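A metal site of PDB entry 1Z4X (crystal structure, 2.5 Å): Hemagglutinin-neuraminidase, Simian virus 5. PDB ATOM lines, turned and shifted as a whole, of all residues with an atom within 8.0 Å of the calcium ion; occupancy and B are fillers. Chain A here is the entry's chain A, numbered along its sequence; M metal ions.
Pro 223 touches the calcium ion.
Along chain A the residues within 4 Å of the calcium ion span positions 217 to 252.
The calcium ion is bound by O of Ala 252, O of Asp 217, O of Ala 222, OG of Ser 220 and O of Ser 220.
The calcium ion has five donor atoms within binding distance.
The backbone carbonyl oxygen of Gly 275 sits at hydrogen-bond distance from the backbone NH of Ala 252 (2.8 Å).
The side-chain hydroxyl (OG1) of Thr 253 sits close to the backbone carbonyl oxygen (O) of Asp 217 (3.2 Å).
The side-chain carboxylate of Asp 217 is in hydrogen-bond range of the side-chain amide nitrogen of Gln 212 (2.9 Å).
The side-chain hydroxyl (OG) of Ser 220 sits close to the backbone carbonyl oxygen (O) of Asp 216 (3.3 Å).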
ATOM      1  N   GLN A 212      16.441   8.020   3.995  1.00  0.00           N
ATOM      2  CA  GLN A 212      15.142   8.352   4.572  1.00  0.00           C
ATOM      3  C   GLN A 212      15.364   8.992   5.946  1.00  0.00           C
ATOM      4  O   GLN A 212      16.448   8.890   6.506  1.00  0.00           O
ATOM      5  CB  GLN A 212      14.326   7.079   4.715  1.00  0.00           C
ATOM      6  CG  GLN A 212      14.901   6.084   5.717  1.00  0.00           C
ATOM      7  CD  GLN A 212      14.247   4.726   5.640  1.00  0.00           C
ATOM      8  OE1 GLN A 212      13.081   4.611   5.287  1.00  0.00           O
ATOM      9  NE2 GLN A 212      14.987   3.694   6.009  1.00  0.00           N
ATOM     10  N   GLU A 214      15.778   9.722   9.797  1.00  0.00           N
ATOM     11  CA  GLU A 214      16.349   8.857  10.810  1.00  0.00           C
ATOM     12  C   GLU A 214      15.335   7.961  11.496  1.00  0.00           C
ATOM     13  O   GLU A 214      15.575   6.763  11.683  1.00  0.00           O
ATOM     14  CB  GLU A 214      17.089   9.695  11.855  1.00  0.00           C
ATOM     15  CG  GLU A 214      17.467   8.930  13.113  1.00  0.00           C
ATOM     16  CD  GLU A 214      18.280   9.755  14.077  1.00  0.00           C
ATOM     17  OE1 GLU A 214      17.906  10.908  14.333  1.00  0.00           O
ATOM     18  OE2 GLU A 214      19.295   9.232  14.590  1.00  0.00           O
ATOM     19  N   ARG A 215      14.195   8.534  11.881  1.00  0.00           N
ATOM     20  CA  ARG A 215      13.176   7.755  12.574  1.00  0.00           C
ATOM     21  C   ARG A 215      12.740   6.561  11.736  1.00  0.00           C
ATOM     22  O   ARG A 215      12.505   5.469  12.269  1.00  0.00           O
ATOM     23  CB  ARG A 215      11.977   8.636  12.901  1.00  0.00           C
ATOM     24  CG  ARG A 215      11.045   7.991  13.894  1.00  0.00           C
ATOM     25  CD  ARG A 215       9.795   8.798  14.082  1.00  0.00           C
ATOM     26  NE  ARG A 215       8.847   8.088  14.928  1.00  0.00           N
ATOM     27  CZ  ARG A 215       7.537   8.301  14.912  1.00  0.00           C
ATOM     28  NH1 ARG A 215       7.028   9.216  14.093  1.00  0.00           N
ATOM     29  NH2 ARG A 215       6.735   7.603  15.705  1.00  0.00           N
ATOM     30  N   ASP A 216      12.640   6.750  10.425  1.00  0.00           N
ATOM     31  CA  ASP A 216      12.238   5.678   9.528  1.00  0.00           C
ATOM     32  C   ASP A 216      13.231   4.531   9.574  1.00  0.00           C
ATOM     33  O   ASP A 216      12.852   3.368   9.396  1.00  0.00           O
ATOM     34  CB  ASP A 216      12.098   6.202   8.096  1.00  0.00           C
ATOM     35  CG  ASP A 216      10.981   7.221   7.949  1.00  0.00           C
ATOM     36  OD1 ASP A 216      10.364   7.580   8.969  1.00  0.00           O
ATOM     37  OD2 ASP A 216      10.725   7.670   6.815  1.00  0.00           O
ATOM     38  N   ASP A 217      14.500   4.841   9.793  1.00  0.00           N
ATOM     39  CA  ASP A 217      15.525   3.801   9.874  1.00  0.00           C
ATOM     40  C   ASP A 217      15.228   2.856  11.033  1.00  0.00           C
ATOM     41  O   ASP A 217      15.467   1.664  10.938  1.00  0.00           O
ATOM     42  CB  ASP A 217      16.918   4.396  10.069  1.00  0.00           C
ATOM     43  CG  ASP A 217      17.485   4.996   8.802  1.00  0.00           C
ATOM     44  OD1 ASP A 217      17.258   4.413   7.722  1.00  0.00           O
ATOM     45  OD2 ASP A 217      18.176   6.025   8.884  1.00  0.00           O
ATOM     46  N   TYR A 218      14.728   3.379  12.134  1.00  0.00           N
ATOM     47  CA  TYR A 218      14.442   2.508  13.270  1.00  0.00           C
ATOM     48  C   TYR A 218      13.224   1.603  13.052  1.00  0.00           C
ATOM     49  O   TYR A 218      13.188   0.487  13.550  1.00  0.00           O
ATOM     50  CB  TYR A 218      14.265   3.342  14.534  1.00  0.00           C
ATOM     51  CG  TYR A 218      15.570   3.919  15.035  1.00  0.00           C
ATOM     52  CD1 TYR A 218      16.132   5.043  14.442  1.00  0.00           C
ATOM     53  CD2 TYR A 218      16.280   3.295  16.070  1.00  0.00           C
ATOM     54  CE1 TYR A 218      17.381   5.524  14.853  1.00  0.00           C
ATOM     55  CE2 TYR A 218      17.522   3.768  16.481  1.00  0.00           C
ATOM     56  CZ  TYR A 218      18.064   4.883  15.870  1.00  0.00           C
ATOM     57  OH  TYR A 218      19.306   5.329  16.250  1.00  0.00           O
ATOM     58  N   PHE A 219      12.230   2.095  12.304  1.00  0.00           N
ATOM     59  CA  PHE A 219      11.045   1.285  12.041  1.00  0.00           C
ATOM     60  C   PHE A 219      11.285   0.190  11.013  1.00  0.00           C
ATOM     61  O   PHE A 219      10.762  -0.922  11.160  1.00  0.00           O
ATOM     62  CB  PHE A 219       9.874   2.166  11.604  1.00  0.00           C
ATOM     63  CG  PHE A 219       9.178   2.837  12.748  1.00  0.00           C
ATOM     64  CD1 PHE A 219       9.663   4.017  13.271  1.00  0.00           C
ATOM     65  CD2 PHE A 219       8.067   2.247  13.344  1.00  0.00           C
ATOM     66  CE1 PHE A 219       9.058   4.614  14.384  1.00  0.00           C
ATOM     67  CE2 PHE A 219       7.452   2.826  14.444  1.00  0.00           C
ATOM     68  CZ  PHE A 219       7.954   4.003  14.971  1.00  0.00           C
ATOM     69  N   SER A 220      12.054   0.479   9.968  1.00  0.00           N
ATOM     70  CA  SER A 220      12.333  -0.542   8.962  1.00  0.00           C
ATOM     71  C   SER A 220      13.218  -1.623   9.589  1.00  0.00           C
ATOM     72  O   SER A 220      14.152  -1.330  10.323  1.00  0.00           O
ATOM     73  CB  SER A 220      13.020   0.080   7.732  1.00  0.00           C
ATOM     74  OG  SER A 220      14.226   0.729   8.057  1.00  0.00           O
ATOM     75  N   ALA A 221      12.895  -2.881   9.330  1.00  0.00           N
ATOM     76  CA  ALA A 221      13.664  -3.987   9.909  1.00  0.00           C
ATOM     77  C   ALA A 221      15.027  -4.143   9.237  1.00  0.00           C
ATOM     78  O   ALA A 221      15.933  -4.783   9.779  1.00  0.00           O
ATOM     79  CB  ALA A 221      12.866  -5.288   9.806  1.00  0.00           C
ATOM     80  N   ALA A 222      15.159  -3.582   8.039  1.00  0.00           N
ATOM     81  CA  ALA A 222      16.418  -3.663   7.303  1.00  0.00           C
ATOM     82  C   ALA A 222      17.314  -2.489   7.663  1.00  0.00           C
ATOM     83  O   ALA A 222      16.870  -1.361   7.647  1.00  0.00           O
ATOM     84  CB  ALA A 222      16.151  -3.671   5.806  1.00  0.00           C
ATOM     85  N   PRO A 223      18.587  -2.742   7.951  1.00  0.00           N
ATOM     86  CA  PRO A 223      19.537  -1.692   8.320  1.00  0.00           C
ATOM     87  C   PRO A 223      20.078  -0.955   7.095  1.00  0.00           C
ATOM     88  O   PRO A 223      20.110  -1.498   6.002  1.00  0.00           O
ATOM     89  CB  PRO A 223      20.621  -2.465   9.038  1.00  0.00           C
ATOM     90  CG  PRO A 223      20.700  -3.713   8.209  1.00  0.00           C
ATOM     91  CD  PRO A 223      19.242  -4.063   7.970  1.00  0.00           C
ATOM     92  N   PRO A 224      20.511   0.309   7.278  1.00  0.00           N
ATOM     93  CA  PRO A 224      21.046   1.091   6.167  1.00  0.00           C
ATOM     94  C   PRO A 224      22.345   0.464   5.682  1.00  0.00           C
ATOM     95  O   PRO A 224      22.982  -0.321   6.382  1.00  0.00           O
ATOM     96  CB  PRO A 224      21.305   2.461   6.788  1.00  0.00           C
ATOM     97  CG  PRO A 224      20.349   2.519   7.927  1.00  0.00           C
ATOM     98  CD  PRO A 224      20.432   1.132   8.497  1.00  0.00           C
ATOM     99  N   TRP A 251      19.994  -5.584  14.117  1.00  0.00           N
ATOM    100  CA  TRP A 251      19.957  -4.127  14.223  1.00  0.00           C
ATOM    101  C   TRP A 251      19.047  -3.530  13.153  1.00  0.00           C
ATOM    102  O   TRP A 251      19.267  -3.738  11.966  1.00  0.00           O
ATOM    103  CB  TRP A 251      21.361  -3.536  14.051  1.00  0.00           C
ATOM    104  CG  TRP A 251      22.357  -3.923  15.106  1.00  0.00           C
ATOM    105  CD1 TRP A 251      22.908  -5.160  15.316  1.00  0.00           C
ATOM    106  CD2 TRP A 251      22.955  -3.043  16.078  1.00  0.00           C
ATOM    107  NE1 TRP A 251      23.806  -5.103  16.358  1.00  0.00           N
ATOM    108  CE2 TRP A 251      23.846  -3.825  16.842  1.00  0.00           C
ATOM    109  CE3 TRP A 251      22.809  -1.679  16.374  1.00  0.00           C
ATOM    110  CZ2 TRP A 251      24.598  -3.276  17.890  1.00  0.00           C
ATOM    111  CZ3 TRP A 251      23.560  -1.144  17.418  1.00  0.00           C
ATOM    112  CH2 TRP A 251      24.445  -1.934  18.159  1.00  0.00           C
ATOM    113  N   ALA A 252      18.026  -2.782  13.557  1.00  0.00           N
ATOM    114  CA  ALA A 252      17.131  -2.145  12.595  1.00  0.00           C
ATOM    115  C   ALA A 252      17.938  -1.022  11.958  1.00  0.00           C
ATOM    116  O   ALA A 252      17.751  -0.695  10.806  1.00  0.00           O
ATOM    117  CB  ALA A 252      15.883  -1.600  13.290  1.00  0.00           C
ATOM    118  N   THR A 253      18.846  -0.426  12.720  1.00  0.00           N
ATOM    119  CA  THR A 253      19.720   0.631  12.195  1.00  0.00           C
ATOM    120  C   THR A 253      21.071   0.519  12.855  1.00  0.00           C
ATOM    121  O   THR A 253      21.193  -0.051  13.938  1.00  0.00           O
ATOM    122  CB  THR A 253      19.242   2.052  12.504  1.00  0.00           C
ATOM    123  OG1 THR A 253      17.894   2.030  12.961  1.00  0.00           O
ATOM    124  CG2 THR A 253      19.375   2.907  11.268  1.00  0.00           C
ATOM    125  N   LEU A 254      22.066   1.097  12.193  1.00  0.00           N
ATOM    126  CA  LEU A 254      23.438   1.093  12.696  1.00  0.00           C
ATOM    127  C   LEU A 254      24.114   2.343  12.141  1.00  0.00           C
ATOM    128  O   LEU A 254      24.063   2.594  10.933  1.00  0.00           O
ATOM    129  CB  LEU A 254      24.153  -0.179  12.219  1.00  0.00           C
ATOM    130  CG  LEU A 254      25.613  -0.379  12.630  1.00  0.00           C
ATOM    131  CD1 LEU A 254      25.755  -0.306  14.143  1.00  0.00           C
ATOM    132  CD2 LEU A 254      26.097  -1.719  12.105  1.00  0.00           C
ATOM    133  N   GLY A 275      19.573   0.819  16.814  1.00  0.00           N
ATOM    134  CA  GLY A 275      18.460   0.174  17.491  1.00  0.00           C
ATOM    135  C   GLY A 275      18.416  -1.313  17.225  1.00  0.00           C
ATOM    136  O   GLY A 275      18.501  -1.752  16.083  1.00  0.00           O
ATOM    137  N   ILE A 277      16.507  -5.069  17.450  1.00  0.00           N
ATOM    138  CA  ILE A 277      15.173  -5.638  17.332  1.00  0.00           C
ATOM    139  C   ILE A 277      14.794  -6.545  18.496  1.00  0.00           C
ATOM    140  O   ILE A 277      15.593  -7.358  18.962  1.00  0.00           O
ATOM    141  CB  ILE A 277      15.067  -6.433  16.016  1.00  0.00           C
ATOM    142  CG1 ILE A 277      15.271  -5.481  14.844  1.00  0.00           C
ATOM    143  CG2 ILE A 277      13.721  -7.146  15.933  1.00  0.00           C
ATOM    144  CD1 ILE A 277      15.364  -6.162  13.501  1.00  0.00           C
ATOM    145  N   ARG A 323      12.784   0.038  19.479  1.00  0.00           N
ATOM    146  CA  ARG A 323      14.062  -0.661  19.438  1.00  0.00           C
ATOM    147  C   ARG A 323      14.864  -0.388  20.699  1.00  0.00           C
ATOM    148  O   ARG A 323      14.622   0.588  21.394  1.00  0.00           O
ATOM    149  CB  ARG A 323      14.912  -0.183  18.253  1.00  0.00           C
ATOM    150  CG  ARG A 323      14.205  -0.170  16.921  1.00  0.00           C
ATOM    151  CD  ARG A 323      13.702  -1.544  16.550  1.00  0.00           C
ATOM    152  NE  ARG A 323      13.159  -1.551  15.195  1.00  0.00           N
ATOM    153  CZ  ARG A 323      12.464  -2.554  14.674  1.00  0.00           C
ATOM    154  NH1 ARG A 323      12.226  -3.646  15.395  1.00  0.00           N
ATOM    155  NH2 ARG A 323      12.021  -2.478  13.423  1.00  0.00           N
HETATM  156 CA    CA M   1      16.086   0.027   9.377  1.00  0.00          CA
